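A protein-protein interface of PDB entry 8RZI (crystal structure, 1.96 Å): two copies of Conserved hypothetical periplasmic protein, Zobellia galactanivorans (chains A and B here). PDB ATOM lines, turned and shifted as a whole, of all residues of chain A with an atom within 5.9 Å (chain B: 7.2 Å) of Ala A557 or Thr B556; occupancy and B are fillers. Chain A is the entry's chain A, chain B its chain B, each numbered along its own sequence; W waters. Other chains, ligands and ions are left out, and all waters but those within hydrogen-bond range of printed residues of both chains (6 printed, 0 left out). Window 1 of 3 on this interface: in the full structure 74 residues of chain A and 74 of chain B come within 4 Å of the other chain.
The backbone NH of Ile B563 lies within hydrogen-bond range of the side-chain carboxylate of Asp B560.
The backbone NH of Asn B558 lies close to the side-chain hydroxyl of Thr B556, at 3.1 Å.
The side-chain carboxylate (OD1) of Asp B550 is in hydrogen-bond range of the side-chain hydroxyl (OG1) of Thr B556 (2.6 Å).
The side-chain amino group of Lys B564 is in hydrogen-bond range of the side-chain hydroxyl of Thr B556, at 3.5 Å.
OG1 of Thr A556 sits at hydrogen-bond distance from OD1 of Asp A550 (2.6 Å).
The backbone carbonyl oxygen (O) of Glu B554 sits at hydrogen-bond distance from the side-chain amino group (NZ) of Lys B564 (2.9 Å).
Of the printed residues of chain B, Lys A182 touches Glu B520 and Gln B549.
Printed residues of chain B within 4 Å of Val A555: Arg B179 (2.8 Å), Val B555 (3.8 Å), Gly B559 (3.8 Å) and Asp B560 (3.6 Å).
Ala A557 touches just these residues of chain B: Thr B556 (3.9 Å) and Ala B557 (3.6 Å).
Of the printed residues of chain A, Arg B179 touches Val A555 and Thr A556.
Printed residues of chain A within 4 Å of Ala B557: Thr A556 and Ala A557.
Of the printed residues of chain A, Gly B559 touches Val A555.
The nearest residue of chain A that does not touch Thr B556 is Val A555 (4.2 Å).
Among the printed residues, Asp or Glu carboxylates within 4 Å of a Lys or Arg side-chain nitrogen of the other chain: Arg A179 with Glu B554 and Lys A182 with Glu B520.
Water W2 lies within hydrogen-bond range of O of Val A555 (2.7 Å), O of Ala B557 (3.0 Å) and N of Gly B559 (3.2 Å).
Water W6 lies within hydrogen-bond range of the backbone carbonyl oxygen (O) of Gln B549 (2.7 Å), the side-chain amino group (NZ) of Lys A182 (2.8 Å) and the guanidinium group (NE) of Arg A179 (3.2 Å).
Water W3 lies within hydrogen-bond range of NE2 of Gln B549 and N of Lys A182.
Water W1 lies within hydrogen-bond range of the side-chain carboxylate (OE1) of Glu B520 (2.9 Å) and the side-chain amino group (NZ) of Lys A182 (3.1 Å).
Water W5 lies within hydrogen-bond range of O of Val B555, O of Ala A557 and N of Gly A559.
Water W4 lies within hydrogen-bond range of the side-chain carboxylate of Glu B554 (3.2 Å) and the guanidinium group of Arg A179 (3.4 Å).
Val A555 touches its own counterpart, Val B555.
Thr A556 touches its own counterpart, Thr B556.
Thr A556 touches Ala B557, and with the chains exchanged Ala A557 touches Thr B556.
Ala A557 touches its own counterpart, Ala B557.
Positions printed for both chains: 179, 520, 550, 555, 556, 557, 558 and 559.
Of the 15 pairs that touch across the chains among the printed residues, 11 have their exchanged pair printed and touching as well.
Thr B556 touches Arg A179 (CG2 to NH2, 3.6 Å).
Val A555 touches Val B555.
Val A555 touches Gly B559 (CG1 to C, 3.8 Å).
CG1 of Val A555 touches N of Asp B560, at 3.6 Å.
CG2 of Thr A556 touches NH2 of Arg B179, 3.6 Å away.
Thr A556 touches Ala B557 (C to N, 3.8 Å).
Ala A557 touches Thr B556 (N to C, 3.9 Å).
N of Ala B557 touches N of Ala A557, at 3.6 Å.
Val B555 touches Gly A559.
The side-chain amino group (NZ) of Lys A182 is in salt-bridge range of the side-chain carboxylate (OE2) of Glu B520.
O of Gln B549 sits close to NZ of Lys A182 (3.5 Å).
OE1 of Glu B554 is in salt-bridge range of NE of Arg A179, at 2.8 Å.
The guanidinium group (NH2) of Arg A179 is in hydrogen-bond range of the backbone carbonyl oxygen (O) of Val B555, 2.9 Å away.
The backbone carbonyl oxygen of Val A555 is in hydrogen-bond range of the guanidinium group of Arg B179 (2.8 Å).
O of Thr B556 lies close to O of Thr A556 (3.4 Å).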
ATOM      1  N   ARG A 179     -12.187   0.053 -33.099  1.00  0.00           N
ATOM      2  CA  ARG A 179     -12.898   0.873 -34.073  1.00  0.00           C
ATOM      3  C   ARG A 179     -11.972   1.339 -35.188  1.00  0.00           C
ATOM      4  O   ARG A 179     -12.377   1.405 -36.353  1.00  0.00           O
ATOM      5  CB  ARG A 179     -13.514   2.086 -33.370  1.00  0.00           C
ATOM      6  CG  ARG A 179     -14.326   1.730 -32.151  1.00  0.00           C
ATOM      7  CD  ARG A 179     -15.678   1.216 -32.630  1.00  0.00           C
ATOM      8  NE  ARG A 179     -16.555   0.867 -31.518  1.00  0.00           N
ATOM      9  CZ  ARG A 179     -17.754   0.322 -31.658  1.00  0.00           C
ATOM     10  NH1 ARG A 179     -18.243   0.085 -32.874  1.00  0.00           N
ATOM     11  NH2 ARG A 179     -18.456   0.031 -30.580  1.00  0.00           N
ATOM     12  N   LYS A 182     -11.358  -1.353 -37.884  1.00  0.00           N
ATOM     13  CA  LYS A 182     -12.559  -1.504 -38.705  1.00  0.00           C
ATOM     14  C   LYS A 182     -12.782  -0.289 -39.606  1.00  0.00           C
ATOM     15  O   LYS A 182     -13.118  -0.440 -40.790  1.00  0.00           O
ATOM     16  CB  LYS A 182     -13.787  -1.730 -37.811  1.00  0.00           C
ATOM     17  CG  LYS A 182     -13.874  -3.145 -37.167  1.00  0.00           C
ATOM     18  CD  LYS A 182     -15.179  -3.298 -36.325  1.00  0.00           C
ATOM     19  CE  LYS A 182     -15.126  -2.513 -35.024  1.00  0.00           C
ATOM     20  NZ  LYS A 182     -16.373  -2.649 -34.182  1.00  0.00           N
ATOM     21  N   GLU A 520     -29.292  -0.996 -36.244  1.00  0.00           N
ATOM     22  CA  GLU A 520     -28.136  -1.585 -35.569  1.00  0.00           C
ATOM     23  C   GLU A 520     -27.043  -1.929 -36.573  1.00  0.00           C
ATOM     24  O   GLU A 520     -25.903  -1.491 -36.429  1.00  0.00           O
ATOM     25  CB  GLU A 520     -28.556  -2.818 -34.772  1.00  0.00           C
ATOM     26  CG  GLU A 520     -29.387  -2.469 -33.531  1.00  0.00           C
ATOM     27  CD  GLU A 520     -30.119  -3.676 -32.972  1.00  0.00           C
ATOM     28  OE1 GLU A 520     -29.417  -4.623 -32.543  1.00  0.00           O
ATOM     29  OE2 GLU A 520     -31.387  -3.692 -33.012  1.00  0.00           O
ATOM     30  N   ASP A 521     -27.383  -2.699 -37.604  1.00  0.00           N
ATOM     31  CA  ASP A 521     -26.473  -3.084 -38.682  1.00  0.00           C
ATOM     32  C   ASP A 521     -26.874  -2.329 -39.937  1.00  0.00           C
ATOM     33  O   ASP A 521     -28.016  -2.455 -40.396  1.00  0.00           O
ATOM     34  CB  ASP A 521     -26.525  -4.589 -38.957  1.00  0.00           C
ATOM     35  CG  ASP A 521     -26.377  -5.409 -37.706  1.00  0.00           C
ATOM     36  OD1 ASP A 521     -25.346  -5.260 -36.982  1.00  0.00           O
ATOM     37  OD2 ASP A 521     -27.303  -6.206 -37.422  1.00  0.00           O
ATOM     38  N   ASP A 550     -34.531  -1.556 -30.672  1.00  0.00           N
ATOM     39  CA  ASP A 550     -33.213  -1.174 -30.166  1.00  0.00           C
ATOM     40  C   ASP A 550     -33.421  -0.202 -29.013  1.00  0.00           C
ATOM     41  O   ASP A 550     -32.962   0.940 -29.048  1.00  0.00           O
ATOM     42  CB  ASP A 550     -32.378  -0.563 -31.302  1.00  0.00           C
ATOM     43  CG  ASP A 550     -30.954  -0.218 -30.895  1.00  0.00           C
ATOM     44  OD1 ASP A 550     -30.453  -0.822 -29.929  1.00  0.00           O
ATOM     45  OD2 ASP A 550     -30.338   0.679 -31.538  1.00  0.00           O
ATOM     46  N   VAL A 555     -28.549  -3.718 -24.909  1.00  0.00           N
ATOM     47  CA  VAL A 555     -27.176  -3.425 -25.308  1.00  0.00           C
ATOM     48  C   VAL A 555     -26.971  -3.916 -26.736  1.00  0.00           C
ATOM     49  O   VAL A 555     -27.082  -5.117 -27.007  1.00  0.00           O
ATOM     50  CB  VAL A 555     -26.174  -4.089 -24.358  1.00  0.00           C
ATOM     51  CG1 VAL A 555     -24.758  -3.785 -24.825  1.00  0.00           C
ATOM     52  CG2 VAL A 555     -26.396  -3.597 -22.901  1.00  0.00           C
ATOM     53  N   THR A 556     -26.659  -3.001 -27.649  1.00  0.00           N
ATOM     54  CA  THR A 556     -26.625  -3.317 -29.079  1.00  0.00           C
ATOM     55  C   THR A 556     -25.436  -2.614 -29.725  1.00  0.00           C
ATOM     56  O   THR A 556     -24.661  -1.913 -29.068  1.00  0.00           O
ATOM     57  CB  THR A 556     -27.912  -2.884 -29.794  1.00  0.00           C
ATOM     58  OG1 THR A 556     -27.969  -1.453 -29.833  1.00  0.00           O
ATOM     59  CG2 THR A 556     -29.144  -3.460 -29.128  1.00  0.00           C
ATOM     60  N   ALA A 557     -25.347  -2.739 -31.050  1.00  0.00           N
ATOM     61  CA  ALA A 557     -24.335  -1.991 -31.785  1.00  0.00           C
ATOM     62  C   ALA A 557     -24.441  -0.495 -31.543  1.00  0.00           C
ATOM     63  O   ALA A 557     -23.444   0.208 -31.703  1.00  0.00           O
ATOM     64  CB  ALA A 557     -24.445  -2.272 -33.276  1.00  0.00           C
ATOM     65  N   ASN A 558     -25.633   0.021 -31.192  1.00  0.00           N
ATOM     66  CA  ASN A 558     -25.799   1.462 -30.992  1.00  0.00           C
ATOM     67  C   ASN A 558     -25.565   1.896 -29.556  1.00  0.00           C
ATOM     68  O   ASN A 558     -25.705   3.087 -29.255  1.00  0.00           O
ATOM     69  CB  ASN A 558     -27.193   1.920 -31.445  1.00  0.00           C
ATOM     70  CG  ASN A 558     -27.340   1.883 -32.952  1.00  0.00           C
ATOM     71  OD1 ASN A 558     -26.447   2.317 -33.686  1.00  0.00           O
ATOM     72  ND2 ASN A 558     -28.442   1.336 -33.421  1.00  0.00           N
ATOM     73  N   GLY A 559     -25.239   0.970 -28.664  1.00  0.00           N
ATOM     74  CA  GLY A 559     -24.762   1.319 -27.338  1.00  0.00           C
ATOM     75  C   GLY A 559     -25.528   0.608 -26.242  1.00  0.00           C
ATOM     76  O   GLY A 559     -26.449  -0.174 -26.485  1.00  0.00           O
ATOM     77  N   ARG B 179     -35.832  -7.765 -28.956  1.00  0.00           N
ATOM     78  CA  ARG B 179     -35.232  -8.965 -29.523  1.00  0.00           C
ATOM     79  C   ARG B 179     -36.297  -9.862 -30.139  1.00  0.00           C
ATOM     80  O   ARG B 179     -36.070 -10.480 -31.184  1.00  0.00           O
ATOM     81  CB  ARG B 179     -34.467  -9.748 -28.442  1.00  0.00           C
ATOM     82  CG  ARG B 179     -33.358  -8.941 -27.730  1.00  0.00           C
ATOM     83  CD  ARG B 179     -32.175  -8.737 -28.653  1.00  0.00           C
ATOM     84  NE  ARG B 179     -31.133  -7.943 -27.999  1.00  0.00           N
ATOM     85  CZ  ARG B 179     -29.996  -7.580 -28.572  1.00  0.00           C
ATOM     86  NH1 ARG B 179     -29.739  -7.965 -29.819  1.00  0.00           N
ATOM     87  NH2 ARG B 179     -29.124  -6.845 -27.893  1.00  0.00           N
ATOM     88  N   LEU B 519     -18.398 -12.520 -34.798  1.00  0.00           N
ATOM     89  CA  LEU B 519     -18.547 -11.275 -35.547  1.00  0.00           C
ATOM     90  C   LEU B 519     -19.627 -10.417 -34.890  1.00  0.00           C
ATOM     91  O   LEU B 519     -20.511 -10.923 -34.198  1.00  0.00           O
ATOM     92  CB  LEU B 519     -18.943 -11.538 -36.998  1.00  0.00           C
ATOM     93  CG  LEU B 519     -17.943 -12.056 -38.006  1.00  0.00           C
ATOM     94  CD1 LEU B 519     -18.606 -11.929 -39.364  1.00  0.00           C
ATOM     95  CD2 LEU B 519     -16.628 -11.232 -37.929  1.00  0.00           C
ATOM     96  N   GLU B 520     -19.546  -9.097 -35.098  1.00  0.00           N
ATOM     97  CA  GLU B 520     -20.592  -8.215 -34.586  1.00  0.00           C
ATOM     98  C   GLU B 520     -21.823  -8.259 -35.492  1.00  0.00           C
ATOM     99  O   GLU B 520     -22.942  -8.461 -35.024  1.00  0.00           O
ATOM    100  CB  GLU B 520     -20.058  -6.780 -34.479  1.00  0.00           C
ATOM    101  CG  GLU B 520     -18.937  -6.626 -33.468  1.00  0.00           C
ATOM    102  CD  GLU B 520     -18.217  -5.288 -33.592  1.00  0.00           C
ATOM    103  OE1 GLU B 520     -18.906  -4.244 -33.492  1.00  0.00           O
ATOM    104  OE2 GLU B 520     -16.988  -5.281 -33.843  1.00  0.00           O
ATOM    105  N   GLN B 549     -10.981  -6.306 -32.567  1.00  0.00           N
ATOM    106  CA  GLN B 549     -11.955  -5.356 -33.115  1.00  0.00           C
ATOM    107  C   GLN B 549     -13.181  -5.208 -32.227  1.00  0.00           C
ATOM    108  O   GLN B 549     -13.886  -4.193 -32.317  1.00  0.00           O
ATOM    109  CB  GLN B 549     -12.418  -5.763 -34.514  1.00  0.00           C
ATOM    110  CG  GLN B 549     -11.440  -5.428 -35.602  1.00  0.00           C
ATOM    111  CD  GLN B 549     -10.508  -6.600 -35.909  1.00  0.00           C
ATOM    112  OE1 GLN B 549     -10.393  -7.545 -35.122  1.00  0.00           O
ATOM    113  NE2 GLN B 549      -9.854  -6.541 -37.057  1.00  0.00           N
ATOM    114  N   ASP B 550     -13.449  -6.199 -31.387  1.00  0.00           N
ATOM    115  CA  ASP B 550     -14.635  -6.252 -30.539  1.00  0.00           C
ATOM    116  C   ASP B 550     -14.211  -6.551 -29.104  1.00  0.00           C
ATOM    117  O   ASP B 550     -14.655  -7.538 -28.501  1.00  0.00           O
ATOM    118  CB  ASP B 550     -15.578  -7.327 -31.077  1.00  0.00           C
ATOM    119  CG  ASP B 550     -16.894  -7.353 -30.379  1.00  0.00           C
ATOM    120  OD1 ASP B 550     -17.239  -6.340 -29.750  1.00  0.00           O
ATOM    121  OD2 ASP B 550     -17.594  -8.392 -30.474  1.00  0.00           O
ATOM    122  N   PRO B 551     -13.346  -5.729 -28.518  1.00  0.00           N
ATOM    123  CA  PRO B 551     -12.712  -6.108 -27.251  1.00  0.00           C
ATOM    124  C   PRO B 551     -13.692  -5.911 -26.098  1.00  0.00           C
ATOM    125  O   PRO B 551     -14.781  -5.371 -26.255  1.00  0.00           O
ATOM    126  CB  PRO B 551     -11.522  -5.148 -27.163  1.00  0.00           C
ATOM    127  CG  PRO B 551     -12.073  -3.876 -27.771  1.00  0.00           C
ATOM    128  CD  PRO B 551     -12.893  -4.392 -28.964  1.00  0.00           C
ATOM    129  N   ASN B 553     -13.629  -3.882 -23.668  1.00  0.00           N
ATOM    130  CA  ASN B 553     -13.815  -2.485 -23.293  1.00  0.00           C
ATOM    131  C   ASN B 553     -14.694  -1.708 -24.267  1.00  0.00           C
ATOM    132  O   ASN B 553     -14.910  -0.516 -24.054  1.00  0.00           O
ATOM    133  CB  ASN B 553     -12.450  -1.782 -23.172  1.00  0.00           C
ATOM    134  CG  ASN B 553     -11.570  -2.003 -24.382  1.00  0.00           C
ATOM    135  OD1 ASN B 553     -11.048  -3.108 -24.584  1.00  0.00           O
ATOM    136  ND2 ASN B 553     -11.368  -0.949 -25.184  1.00  0.00           N
ATOM    137  N   GLU B 554     -15.179  -2.332 -25.334  1.00  0.00           N
ATOM    138  CA  GLU B 554     -16.038  -1.661 -26.309  1.00  0.00           C
ATOM    139  C   GLU B 554     -17.466  -2.173 -26.178  1.00  0.00           C
ATOM    140  O   GLU B 554     -17.683  -3.361 -25.926  1.00  0.00           O
ATOM    141  CB  GLU B 554     -15.533  -1.883 -27.742  1.00  0.00           C
ATOM    142  CG  GLU B 554     -14.396  -0.931 -28.152  1.00  0.00           C
ATOM    143  CD  GLU B 554     -14.847   0.527 -28.183  1.00  0.00           C
ATOM    144  OE1 GLU B 554     -15.875   0.818 -28.819  1.00  0.00           O
ATOM    145  OE2 GLU B 554     -14.194   1.385 -27.534  1.00  0.00           O
ATOM    146  N   VAL B 555     -18.445  -1.286 -26.359  1.00  0.00           N
ATOM    147  CA  VAL B 555     -19.852  -1.684 -26.340  1.00  0.00           C
ATOM    148  C   VAL B 555     -20.298  -1.962 -27.768  1.00  0.00           C
ATOM    149  O   VAL B 555     -20.245  -1.078 -28.622  1.00  0.00           O
ATOM    150  CB  VAL B 555     -20.736  -0.600 -25.701  1.00  0.00           C
ATOM    151  CG1 VAL B 555     -22.191  -1.099 -25.637  1.00  0.00           C
ATOM    152  CG2 VAL B 555     -20.208  -0.220 -24.325  1.00  0.00           C
ATOM    153  N   THR B 556     -20.729  -3.190 -28.044  1.00  0.00           N
ATOM    154  CA  THR B 556     -21.029  -3.565 -29.425  1.00  0.00           C
ATOM    155  C   THR B 556     -22.264  -4.455 -29.441  1.00  0.00           C
ATOM    156  O   THR B 556     -22.877  -4.730 -28.406  1.00  0.00           O
ATOM    157  CB  THR B 556     -19.859  -4.298 -30.113  1.00  0.00           C
ATOM    158  OG1 THR B 556     -19.739  -5.608 -29.562  1.00  0.00           O
ATOM    159  CG2 THR B 556     -18.519  -3.559 -29.933  1.00  0.00           C
ATOM    160  N   ALA B 557     -22.593  -4.947 -30.635  1.00  0.00           N
ATOM    161  CA  ALA B 557     -23.681  -5.900 -30.771  1.00  0.00           C
ATOM    162  C   ALA B 557     -23.507  -7.105 -29.848  1.00  0.00           C
ATOM    163  O   ALA B 557     -24.500  -7.700 -29.425  1.00  0.00           O
ATOM    164  CB  ALA B 557     -23.789  -6.352 -32.232  1.00  0.00           C
ATOM    165  N   ASN B 558     -22.263  -7.482 -29.531  1.00  0.00           N
ATOM    166  CA  ASN B 558     -21.974  -8.641 -28.693  1.00  0.00           C
ATOM    167  C   ASN B 558     -21.942  -8.319 -27.209  1.00  0.00           C
ATOM    168  O   ASN B 558     -21.699  -9.229 -26.405  1.00  0.00           O
ATOM    169  CB  ASN B 558     -20.651  -9.276 -29.122  1.00  0.00           C
ATOM    170  CG  ASN B 558     -20.765  -9.914 -30.477  1.00  0.00           C
ATOM    171  OD1 ASN B 558     -21.778 -10.542 -30.772  1.00  0.00           O
ATOM    172  ND2 ASN B 558     -19.754  -9.746 -31.312  1.00  0.00           N
ATOM    173  N   GLY B 559     -22.178  -7.069 -26.831  1.00  0.00           N
ATOM    174  CA  GLY B 559     -22.406  -6.720 -25.446  1.00  0.00           C
ATOM    175  C   GLY B 559     -21.473  -5.626 -24.959  1.00  0.00           C
ATOM    176  O   GLY B 559     -20.617  -5.126 -25.682  1.00  0.00           O
ATOM    177  N   ASP B 560     -21.668  -5.260 -23.700  1.00  0.00           N
ATOM    178  CA  ASP B 560     -20.818  -4.338 -22.967  1.00  0.00           C
ATOM    179  C   ASP B 560     -19.867  -5.171 -22.117  1.00  0.00           C
ATOM    180  O   ASP B 560     -19.787  -6.394 -22.278  1.00  0.00           O
ATOM    181  CB  ASP B 560     -21.683  -3.381 -22.126  1.00  0.00           C
ATOM    182  CG  ASP B 560     -22.593  -4.118 -21.149  1.00  0.00           C
ATOM    183  OD1 ASP B 560     -22.513  -5.359 -21.073  1.00  0.00           O
ATOM    184  OD2 ASP B 560     -23.406  -3.467 -20.484  1.00  0.00           O
ATOM    185  N   PHE B 561     -19.186  -4.530 -21.165  1.00  0.00           N
ATOM    186  CA  PHE B 561     -18.259  -5.277 -20.327  1.00  0.00           C
ATOM    187  C   PHE B 561     -18.988  -6.292 -19.438  1.00  0.00           C
ATOM    188  O   PHE B 561     -18.491  -7.404 -19.233  1.00  0.00           O
ATOM    189  CB  PHE B 561     -17.422  -4.324 -19.470  1.00  0.00           C
ATOM    190  CG  PHE B 561     -16.366  -5.038 -18.670  1.00  0.00           C
ATOM    191  CD1 PHE B 561     -15.189  -5.430 -19.268  1.00  0.00           C
ATOM    192  CD2 PHE B 561     -16.574  -5.352 -17.338  1.00  0.00           C
ATOM    193  CE1 PHE B 561     -14.217  -6.102 -18.550  1.00  0.00           C
ATOM    194  CE2 PHE B 561     -15.604  -6.015 -16.617  1.00  0.00           C
ATOM    195  CZ  PHE B 561     -14.433  -6.393 -17.229  1.00  0.00           C
ATOM    196  N   ILE B 563     -21.760  -8.050 -19.982  1.00  0.00           N
ATOM    197  CA  ILE B 563     -22.082  -9.241 -20.752  1.00  0.00           C
ATOM    198  C   ILE B 563     -20.814  -9.980 -21.159  1.00  0.00           C
ATOM    199  O   ILE B 563     -20.734 -11.210 -21.045  1.00  0.00           O
ATOM    200  CB  ILE B 563     -22.934  -8.855 -21.977  1.00  0.00           C
ATOM    201  CG1 ILE B 563     -24.283  -8.305 -21.486  1.00  0.00           C
ATOM    202  CG2 ILE B 563     -23.085 -10.065 -22.932  1.00  0.00           C
ATOM    203  CD1 ILE B 563     -25.093  -7.477 -22.511  1.00  0.00           C
ATOM    204  N   LYS B 564     -19.807  -9.248 -21.656  1.00  0.00           N
ATOM    205  CA  LYS B 564     -18.644  -9.937 -22.207  1.00  0.00           C
ATOM    206  C   LYS B 564     -17.843 -10.644 -21.121  1.00  0.00           C
ATOM    207  O   LYS B 564     -17.316 -11.737 -21.351  1.00  0.00           O
ATOM    208  CB  LYS B 564     -17.765  -8.956 -22.969  1.00  0.00           C
ATOM    209  CG  LYS B 564     -18.350  -8.606 -24.331  1.00  0.00           C
ATOM    210  CD  LYS B 564     -17.602  -7.479 -24.984  1.00  0.00           C
ATOM    211  CE  LYS B 564     -18.121  -7.250 -26.389  1.00  0.00           C
ATOM    212  NZ  LYS B 564     -17.447  -6.053 -27.009  1.00  0.00           N
HETATM  213  O   HOH W   1     -18.995  -2.578 -35.815  1.00  0.00           O
HETATM  214  O   HOH W   2     -25.397  -7.227 -26.593  1.00  0.00           O
HETATM  215  O   HOH W   3     -10.564  -4.505 -38.846  1.00  0.00           O
HETATM  216  O   HOH W   4     -15.667   3.748 -30.007  1.00  0.00           O
HETATM  217  O   HOH W   5     -21.949   1.194 -28.997  1.00  0.00           O
HETATM  218  O   HOH W   6     -15.538  -2.140 -31.565  1.00  0.00           O
